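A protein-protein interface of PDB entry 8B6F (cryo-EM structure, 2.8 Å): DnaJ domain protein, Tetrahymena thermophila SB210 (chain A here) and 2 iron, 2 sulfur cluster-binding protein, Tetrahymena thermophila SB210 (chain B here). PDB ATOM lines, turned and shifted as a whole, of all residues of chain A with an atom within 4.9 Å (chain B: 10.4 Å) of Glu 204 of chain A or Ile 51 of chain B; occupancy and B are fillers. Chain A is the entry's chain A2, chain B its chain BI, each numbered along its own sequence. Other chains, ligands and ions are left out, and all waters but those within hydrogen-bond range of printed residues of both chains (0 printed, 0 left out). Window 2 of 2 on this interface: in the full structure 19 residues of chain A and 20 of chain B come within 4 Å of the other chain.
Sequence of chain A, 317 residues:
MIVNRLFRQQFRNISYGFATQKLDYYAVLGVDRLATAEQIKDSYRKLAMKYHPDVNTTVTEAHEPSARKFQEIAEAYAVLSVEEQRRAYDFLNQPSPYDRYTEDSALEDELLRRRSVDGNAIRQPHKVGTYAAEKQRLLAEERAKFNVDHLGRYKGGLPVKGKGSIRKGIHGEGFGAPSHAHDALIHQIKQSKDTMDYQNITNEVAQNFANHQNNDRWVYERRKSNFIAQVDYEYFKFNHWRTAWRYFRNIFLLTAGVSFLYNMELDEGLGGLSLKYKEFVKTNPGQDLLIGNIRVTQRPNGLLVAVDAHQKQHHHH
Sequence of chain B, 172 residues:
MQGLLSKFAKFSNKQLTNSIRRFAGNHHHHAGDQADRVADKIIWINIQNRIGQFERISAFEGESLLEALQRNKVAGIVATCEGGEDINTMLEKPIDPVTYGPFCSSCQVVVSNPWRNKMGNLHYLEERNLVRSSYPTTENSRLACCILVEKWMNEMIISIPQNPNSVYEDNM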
ATOM      1  N   ASP A 183     -27.552 -36.810  -1.821  1.00  0.00           N
ATOM      2  CA  ASP A 183     -27.495 -36.179  -0.509  1.00  0.00           C
ATOM      3  C   ASP A 183     -27.131 -37.227   0.533  1.00  0.00           C
ATOM      4  O   ASP A 183     -27.866 -38.202   0.718  1.00  0.00           O
ATOM      5  CB  ASP A 183     -28.831 -35.520  -0.168  1.00  0.00           C
ATOM      6  CG  ASP A 183     -28.734 -34.584   1.019  1.00  0.00           C
ATOM      7  OD1 ASP A 183     -27.788 -34.730   1.817  1.00  0.00           O
ATOM      8  OD2 ASP A 183     -29.607 -33.703   1.157  1.00  0.00           O
ATOM      9  N   LEU A 185     -27.050 -36.907   3.816  1.00  0.00           N
ATOM     10  CA  LEU A 185     -27.994 -36.910   4.930  1.00  0.00           C
ATOM     11  C   LEU A 185     -29.255 -37.688   4.582  1.00  0.00           C
ATOM     12  O   LEU A 185     -29.771 -38.448   5.410  1.00  0.00           O
ATOM     13  CB  LEU A 185     -28.343 -35.477   5.333  1.00  0.00           C
ATOM     14  CG  LEU A 185     -29.342 -35.341   6.487  1.00  0.00           C
ATOM     15  CD1 LEU A 185     -28.863 -36.089   7.722  1.00  0.00           C
ATOM     16  CD2 LEU A 185     -29.589 -33.881   6.818  1.00  0.00           C
ATOM     17  N   THR A 202     -20.405 -33.885  10.751  1.00  0.00           N
ATOM     18  CA  THR A 202     -20.162 -33.669   9.337  1.00  0.00           C
ATOM     19  C   THR A 202     -19.845 -32.197   9.084  1.00  0.00           C
ATOM     20  O   THR A 202     -19.865 -31.364   9.994  1.00  0.00           O
ATOM     21  CB  THR A 202     -21.369 -34.118   8.514  1.00  0.00           C
ATOM     22  OG1 THR A 202     -22.537 -33.412   8.951  1.00  0.00           O
ATOM     23  CG2 THR A 202     -21.595 -35.609   8.670  1.00  0.00           C
ATOM     24  N   ASN A 203     -19.546 -31.867   7.827  1.00  0.00           N
ATOM     25  CA  ASN A 203     -19.320 -30.470   7.473  1.00  0.00           C
ATOM     26  C   ASN A 203     -20.564 -29.633   7.740  1.00  0.00           C
ATOM     27  O   ASN A 203     -20.466 -28.488   8.194  1.00  0.00           O
ATOM     28  CB  ASN A 203     -18.906 -30.357   6.006  1.00  0.00           C
ATOM     29  CG  ASN A 203     -17.503 -30.863   5.756  1.00  0.00           C
ATOM     30  OD1 ASN A 203     -17.008 -31.731   6.472  1.00  0.00           O
ATOM     31  ND2 ASN A 203     -16.853 -30.320   4.738  1.00  0.00           N
ATOM     32  N   GLU A 204     -21.744 -30.185   7.455  1.00  0.00           N
ATOM     33  CA  GLU A 204     -22.979 -29.457   7.723  1.00  0.00           C
ATOM     34  C   GLU A 204     -23.143 -29.181   9.211  1.00  0.00           C
ATOM     35  O   GLU A 204     -23.520 -28.072   9.606  1.00  0.00           O
ATOM     36  CB  GLU A 204     -24.174 -30.249   7.195  1.00  0.00           C
ATOM     37  CG  GLU A 204     -25.512 -29.566   7.417  1.00  0.00           C
ATOM     38  CD  GLU A 204     -26.674 -30.411   6.947  1.00  0.00           C
ATOM     39  OE1 GLU A 204     -26.429 -31.450   6.299  1.00  0.00           O
ATOM     40  OE2 GLU A 204     -27.832 -30.041   7.231  1.00  0.00           O
ATOM     41  N   VAL A 205     -22.876 -30.180  10.054  1.00  0.00           N
ATOM     42  CA  VAL A 205     -23.013 -29.985  11.495  1.00  0.00           C
ATOM     43  C   VAL A 205     -22.004 -28.959  11.987  1.00  0.00           C
ATOM     44  O   VAL A 205     -22.329 -28.087  12.800  1.00  0.00           O
ATOM     45  CB  VAL A 205     -22.861 -31.327  12.235  1.00  0.00           C
ATOM     46  CG1 VAL A 205     -22.912 -31.119  13.742  1.00  0.00           C
ATOM     47  CG2 VAL A 205     -23.941 -32.296  11.798  1.00  0.00           C
ATOM     48  N   ALA A 206     -20.764 -29.049  11.508  1.00  0.00           N
ATOM     49  CA  ALA A 206     -19.748 -28.087  11.917  1.00  0.00           C
ATOM     50  C   ALA A 206     -20.128 -26.676  11.493  1.00  0.00           C
ATOM     51  O   ALA A 206     -19.952 -25.721  12.256  1.00  0.00           O
ATOM     52  CB  ALA A 206     -18.391 -28.476  11.332  1.00  0.00           C
ATOM     53  N   GLN A 207     -20.658 -26.526  10.279  1.00  0.00           N
ATOM     54  CA  GLN A 207     -21.047 -25.204   9.804  1.00  0.00           C
ATOM     55  C   GLN A 207     -22.247 -24.672  10.576  1.00  0.00           C
ATOM     56  O   GLN A 207     -22.333 -23.468  10.843  1.00  0.00           O
ATOM     57  CB  GLN A 207     -21.342 -25.249   8.307  1.00  0.00           C
ATOM     58  CG  GLN A 207     -21.741 -23.905   7.719  1.00  0.00           C
ATOM     59  CD  GLN A 207     -20.766 -22.799   8.075  1.00  0.00           C
ATOM     60  OE1 GLN A 207     -21.168 -21.685   8.404  1.00  0.00           O
ATOM     61  NE2 GLN A 207     -19.475 -23.103   8.011  1.00  0.00           N
ATOM     62  N   ASN A 208     -23.187 -25.546  10.940  1.00  0.00           N
ATOM     63  CA  ASN A 208     -24.302 -25.110  11.773  1.00  0.00           C
ATOM     64  C   ASN A 208     -23.807 -24.622  13.126  1.00  0.00           C
ATOM     65  O   ASN A 208     -24.282 -23.602  13.638  1.00  0.00           O
ATOM     66  CB  ASN A 208     -25.308 -26.246  11.952  1.00  0.00           C
ATOM     67  CG  ASN A 208     -25.955 -26.664  10.650  1.00  0.00           C
ATOM     68  OD1 ASN A 208     -26.001 -25.896   9.690  1.00  0.00           O
ATOM     69  ND2 ASN A 208     -26.471 -27.885  10.614  1.00  0.00           N
ATOM     70  N   ILE B  47     -16.444 -28.558  -6.095  1.00  0.00           N
ATOM     71  CA  ILE B  47     -17.365 -27.635  -5.449  1.00  0.00           C
ATOM     72  C   ILE B  47     -17.679 -28.137  -4.048  1.00  0.00           C
ATOM     73  O   ILE B  47     -17.800 -29.346  -3.824  1.00  0.00           O
ATOM     74  CB  ILE B  47     -18.667 -27.479  -6.262  1.00  0.00           C
ATOM     75  CG1 ILE B  47     -18.348 -27.028  -7.690  1.00  0.00           C
ATOM     76  CG2 ILE B  47     -19.597 -26.489  -5.585  1.00  0.00           C
ATOM     77  CD1 ILE B  47     -19.534 -27.070  -8.629  1.00  0.00           C
ATOM     78  N   GLN B  48     -17.803 -27.206  -3.107  1.00  0.00           N
ATOM     79  CA  GLN B  48     -18.365 -27.479  -1.790  1.00  0.00           C
ATOM     80  C   GLN B  48     -19.791 -26.942  -1.786  1.00  0.00           C
ATOM     81  O   GLN B  48     -20.006 -25.727  -1.852  1.00  0.00           O
ATOM     82  CB  GLN B  48     -17.537 -26.847  -0.677  1.00  0.00           C
ATOM     83  CG  GLN B  48     -17.957 -27.321   0.706  1.00  0.00           C
ATOM     84  CD  GLN B  48     -17.216 -26.619   1.817  1.00  0.00           C
ATOM     85  OE1 GLN B  48     -16.647 -25.546   1.620  1.00  0.00           O
ATOM     86  NE2 GLN B  48     -17.219 -27.220   3.000  1.00  0.00           N
ATOM     87  N   ASN B  49     -20.758 -27.848  -1.699  1.00  0.00           N
ATOM     88  CA  ASN B  49     -22.160 -27.491  -1.813  1.00  0.00           C
ATOM     89  C   ASN B  49     -22.616 -26.690  -0.594  1.00  0.00           C
ATOM     90  O   ASN B  49     -21.926 -26.595   0.424  1.00  0.00           O
ATOM     91  CB  ASN B  49     -23.007 -28.753  -1.972  1.00  0.00           C
ATOM     92  CG  ASN B  49     -24.411 -28.456  -2.448  1.00  0.00           C
ATOM     93  OD1 ASN B  49     -24.693 -27.366  -2.947  1.00  0.00           O
ATOM     94  ND2 ASN B  49     -25.303 -29.428  -2.301  1.00  0.00           N
ATOM     95  N   ARG B  50     -23.805 -26.096  -0.717  1.00  0.00           N
ATOM     96  CA  ARG B  50     -24.383 -25.327   0.378  1.00  0.00           C
ATOM     97  C   ARG B  50     -24.612 -26.175   1.620  1.00  0.00           C
ATOM     98  O   ARG B  50     -24.718 -25.624   2.720  1.00  0.00           O
ATOM     99  CB  ARG B  50     -25.703 -24.697  -0.066  1.00  0.00           C
ATOM    100  CG  ARG B  50     -26.746 -25.713  -0.493  1.00  0.00           C
ATOM    101  CD  ARG B  50     -27.917 -25.063  -1.203  1.00  0.00           C
ATOM    102  NE  ARG B  50     -28.874 -26.059  -1.666  1.00  0.00           N
ATOM    103  CZ  ARG B  50     -29.962 -25.786  -2.374  1.00  0.00           C
ATOM    104  NH1 ARG B  50     -30.266 -24.548  -2.724  1.00  0.00           N
ATOM    105  NH2 ARG B  50     -30.762 -26.781  -2.742  1.00  0.00           N
ATOM    106  N   ILE B  51     -24.696 -27.497   1.473  1.00  0.00           N
ATOM    107  CA  ILE B  51     -24.924 -28.394   2.600  1.00  0.00           C
ATOM    108  C   ILE B  51     -23.627 -29.033   3.086  1.00  0.00           C
ATOM    109  O   ILE B  51     -23.666 -30.014   3.833  1.00  0.00           O
ATOM    110  CB  ILE B  51     -25.966 -29.472   2.254  1.00  0.00           C
ATOM    111  CG1 ILE B  51     -25.496 -30.312   1.064  1.00  0.00           C
ATOM    112  CG2 ILE B  51     -27.310 -28.819   1.970  1.00  0.00           C
ATOM    113  CD1 ILE B  51     -26.433 -31.443   0.691  1.00  0.00           C
ATOM    114  N   GLY B  52     -22.477 -28.503   2.673  1.00  0.00           N
ATOM    115  CA  GLY B  52     -21.199 -28.949   3.182  1.00  0.00           C
ATOM    116  C   GLY B  52     -20.624 -30.178   2.516  1.00  0.00           C
ATOM    117  O   GLY B  52     -19.541 -30.624   2.916  1.00  0.00           O
ATOM    118  N   GLN B  53     -21.296 -30.741   1.520  1.00  0.00           N
ATOM    119  CA  GLN B  53     -20.783 -31.911   0.829  1.00  0.00           C
ATOM    120  C   GLN B  53     -19.925 -31.486  -0.359  1.00  0.00           C
ATOM    121  O   GLN B  53     -19.820 -30.305  -0.693  1.00  0.00           O
ATOM    122  CB  GLN B  53     -21.935 -32.806   0.381  1.00  0.00           C
ATOM    123  CG  GLN B  53     -22.765 -33.322   1.540  1.00  0.00           C
ATOM    124  CD  GLN B  53     -23.977 -34.097   1.086  1.00  0.00           C
ATOM    125  OE1 GLN B  53     -23.998 -34.656  -0.008  1.00  0.00           O
ATOM    126  NE2 GLN B  53     -25.003 -34.130   1.927  1.00  0.00           N
ATOM    127  N   PHE B  54     -19.313 -32.472  -1.009  1.00  0.00           N
ATOM    128  CA  PHE B  54     -18.380 -32.230  -2.100  1.00  0.00           C
ATOM    129  C   PHE B  54     -18.954 -32.743  -3.412  1.00  0.00           C
ATOM    130  O   PHE B  54     -19.563 -33.816  -3.459  1.00  0.00           O
ATOM    131  CB  PHE B  54     -17.035 -32.907  -1.827  1.00  0.00           C
ATOM    132  CG  PHE B  54     -16.383 -32.459  -0.555  1.00  0.00           C
ATOM    133  CD1 PHE B  54     -16.036 -31.133  -0.371  1.00  0.00           C
ATOM    134  CD2 PHE B  54     -16.107 -33.364   0.453  1.00  0.00           C
ATOM    135  CE1 PHE B  54     -15.436 -30.717   0.798  1.00  0.00           C
ATOM    136  CE2 PHE B  54     -15.506 -32.953   1.625  1.00  0.00           C
ATOM    137  CZ  PHE B  54     -15.169 -31.627   1.796  1.00  0.00           C
ATOM    138  N   GLU B  55     -18.754 -31.970  -4.475  1.00  0.00           N
ATOM    139  CA  GLU B  55     -19.224 -32.323  -5.803  1.00  0.00           C
ATOM    140  C   GLU B  55     -18.107 -32.102  -6.811  1.00  0.00           C
ATOM    141  O   GLU B  55     -17.219 -31.273  -6.605  1.00  0.00           O
ATOM    142  CB  GLU B  55     -20.449 -31.494  -6.203  1.00  0.00           C
ATOM    143  CG  GLU B  55     -21.550 -31.482  -5.158  1.00  0.00           C
ATOM    144  CD  GLU B  55     -22.794 -30.760  -5.632  1.00  0.00           C
ATOM    145  OE1 GLU B  55     -22.949 -30.587  -6.859  1.00  0.00           O
ATOM    146  OE2 GLU B  55     -23.615 -30.364  -4.779  1.00  0.00           O
ATOM    147  N   VAL B  74     -26.061 -27.917 -10.434  1.00  0.00           N
ATOM    148  CA  VAL B  74     -25.496 -27.697  -9.108  1.00  0.00           C
ATOM    149  C   VAL B  74     -26.431 -26.790  -8.322  1.00  0.00           C
ATOM    150  O   VAL B  74     -26.827 -25.720  -8.797  1.00  0.00           O
ATOM    151  CB  VAL B  74     -24.085 -27.094  -9.211  1.00  0.00           C
ATOM    152  CG1 VAL B  74     -23.572 -26.667  -7.841  1.00  0.00           C
ATOM    153  CG2 VAL B  74     -23.135 -28.092  -9.843  1.00  0.00           C
ATOM    154  N   ALA B  75     -26.790 -27.220  -7.117  1.00  0.00           N
ATOM    155  CA  ALA B  75     -27.697 -26.454  -6.282  1.00  0.00           C
ATOM    156  C   ALA B  75     -26.962 -25.303  -5.604  1.00  0.00           C
ATOM    157  O   ALA B  75     -25.737 -25.304  -5.470  1.00  0.00           O
ATOM    158  CB  ALA B  75     -28.341 -27.353  -5.229  1.00  0.00           C
ATOM    159  N   GLY B  76     -27.736 -24.311  -5.172  1.00  0.00           N
ATOM    160  CA  GLY B  76     -27.202 -23.163  -4.471  1.00  0.00           C
ATOM    161  C   GLY B  76     -27.033 -21.918  -5.311  1.00  0.00           C
ATOM    162  O   GLY B  76     -26.582 -20.896  -4.782  1.00  0.00           O
ATOM    163  N   ILE B  77     -27.383 -21.965  -6.594  1.00  0.00           N
ATOM    164  CA  ILE B  77     -27.278 -20.822  -7.491  1.00  0.00           C
ATOM    165  C   ILE B  77     -28.664 -20.518  -8.035  1.00  0.00           C
ATOM    166  O   ILE B  77     -29.317 -21.396  -8.610  1.00  0.00           O
ATOM    167  CB  ILE B  77     -26.282 -21.089  -8.634  1.00  0.00           C
ATOM    168  CG1 ILE B  77     -24.852 -21.007  -8.098  1.00  0.00           C
ATOM    169  CG2 ILE B  77     -26.489 -20.106  -9.789  1.00  0.00           C
ATOM    170  CD1 ILE B  77     -23.803 -21.442  -9.082  1.00  0.00           C
ATOM    171  N   SER B 159     -16.569 -22.834  -3.528  1.00  0.00           N
ATOM    172  CA  SER B 159     -17.649 -23.090  -2.587  1.00  0.00           C
ATOM    173  C   SER B 159     -18.871 -22.309  -3.037  1.00  0.00           C
ATOM    174  O   SER B 159     -18.744 -21.190  -3.539  1.00  0.00           O
ATOM    175  CB  SER B 159     -17.267 -22.689  -1.157  1.00  0.00           C
ATOM    176  OG  SER B 159     -16.113 -23.382  -0.718  1.00  0.00           O
ATOM    177  N   ILE B 160     -20.050 -22.896  -2.862  1.00  0.00           N
ATOM    178  CA  ILE B 160     -21.278 -22.262  -3.332  1.00  0.00           C
ATOM    179  C   ILE B 160     -22.296 -22.200  -2.199  1.00  0.00           C
ATOM    180  O   ILE B 160     -23.178 -23.066  -2.111  1.00  0.00           O
ATOM    181  CB  ILE B 160     -21.857 -23.000  -4.548  1.00  0.00           C
ATOM    182  CG1 ILE B 160     -20.799 -23.090  -5.651  1.00  0.00           C
ATOM    183  CG2 ILE B 160     -23.106 -22.284  -5.049  1.00  0.00           C
ATOM    184  CD1 ILE B 160     -21.265 -23.777  -6.919  1.00  0.00           C
ATOM    185  N   PRO B 161     -22.212 -21.213  -1.312  1.00  0.00           N
ATOM    186  CA  PRO B 161     -23.306 -20.979  -0.363  1.00  0.00           C
ATOM    187  C   PRO B 161     -24.584 -20.605  -1.098  1.00  0.00           C
ATOM    188  O   PRO B 161     -24.606 -20.414  -2.315  1.00  0.00           O
ATOM    189  CB  PRO B 161     -22.789 -19.829   0.507  1.00  0.00           C
ATOM    190  CG  PRO B 161     -21.308 -19.870   0.355  1.00  0.00           C
ATOM    191  CD  PRO B 161     -21.055 -20.345  -1.041  1.00  0.00           C
ATOM    192  N   GLN B 162     -25.669 -20.501  -0.339  1.00  0.00           N
ATOM    193  CA  GLN B 162     -26.955 -20.166  -0.934  1.00  0.00           C
ATOM    194  C   GLN B 162     -27.009 -18.689  -1.298  1.00  0.00           C
ATOM    195  O   GLN B 162     -26.600 -17.824  -0.520  1.00  0.00           O
ATOM    196  CB  GLN B 162     -28.093 -20.510   0.024  1.00  0.00           C
ATOM    197  CG  GLN B 162     -29.476 -20.301  -0.567  1.00  0.00           C
ATOM    198  CD  GLN B 162     -29.722 -21.165  -1.783  1.00  0.00           C
ATOM    199  OE1 GLN B 162     -29.191 -22.267  -1.887  1.00  0.00           O
ATOM    200  NE2 GLN B 162     -30.524 -20.665  -2.715  1.00  0.00           N
ATOM    201  N   ASN B 163     -27.515 -18.404  -2.494  1.00  0.00           N
ATOM    202  CA  ASN B 163     -27.681 -17.043  -2.975  1.00  0.00           C
ATOM    203  C   ASN B 163     -29.077 -16.528  -2.656  1.00  0.00           C
ATOM    204  O   ASN B 163     -30.015 -17.309  -2.473  1.00  0.00           O
ATOM    205  CB  ASN B 163     -27.441 -16.988  -4.479  1.00  0.00           C
ATOM    206  CG  ASN B 163     -26.004 -17.272  -4.846  1.00  0.00           C
ATOM    207  OD1 ASN B 163     -25.087 -16.956  -4.094  1.00  0.00           O
ATOM    208  ND2 ASN B 163     -25.801 -17.880  -6.005  1.00  0.00           N
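OD1 of Asp 183 of chain A sits at hydrogen-bond distance from NE2 of Gln 53 of chain B, 2.9 Å away. The side-chain amide nitrogen of Asn 203 of chain A sits close to the backbone carbonyl oxygen of Gly 52 of chain B, at 3.3 Å.
Ile 51 of chain B touches Asp 183 of chain A. N of Leu 185 of chain A touches NE2 of Gln 53 of chain B, at 3.9 Å. Asn 203 of chain A touches Gln 48 of chain B. ND2 of Asn 203 of chain A touches CZ of Phe 54 of chain B, at 3.6 Å. Glu 204 of chain A touches Ile 51 of chain B.
The side-chain carboxylate of Asp 183 of chain A is in hydrogen-bond range of the backbone NH of Leu 185 of chain A, at 3.0 Å. The backbone carbonyl oxygen (O) of Glu 204 of chain A lies close to the side-chain amide nitrogen (ND2) of Asn 208 of chain A (3.1 Å). OE1 of Gln 48 of chain B sits at hydrogen-bond distance from OG of Ser 159 of chain B (3.2 Å). The backbone NH (N) of Ile 160 of chain B sits at hydrogen-bond distance from the backbone carbonyl oxygen (O) of Gln 48 of chain B, at 3.0 Å.
Of chain B, only Ile 51 (3.4 Å) comes within 4 Å of Glu 204 of chain A. No residue of chain B comes within 4 Å of Thr 202 of chain A. Asn 203 of chain A touches just these residues of chain B: Gln 48, Gly 52 and Phe 54. No residue of chain B comes within 4 Å of Val 205 of chain A. Of the printed residues of chain A, Gln 48 of chain B touches Asn 203. Printed residues of chain A within 4 Å of Gln 53 of chain B: Asp 183 and Leu 185. Of the printed residues of chain B, Leu 185 of chain A touches Gln 53. Gln 207 of chain A touches none of the printed residues of chain B. The nearest printed residue of chain A that does not touch Ile 51 of chain B is Asn 203 of chain A (5.0 Å).
Of the 9 printed residues of chain A, 4 touch a printed residue of chain B. Of the 18 printed residues of chain B, 5 touch a printed residue of chain A. Printed residues of chain B that touch a printed residue of chain A: Gln 48, Ile 51, Gly 52, Gln 53 and Phe 54. Hydrophobic or aromatic side chains of chain B that line the printed part of chain A: Ile 51 and Phe 54. Among the printed residues, no Asp or Glu carboxylate lies within 4 Å of a Lys or Arg side-chain nitrogen of the other chain.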
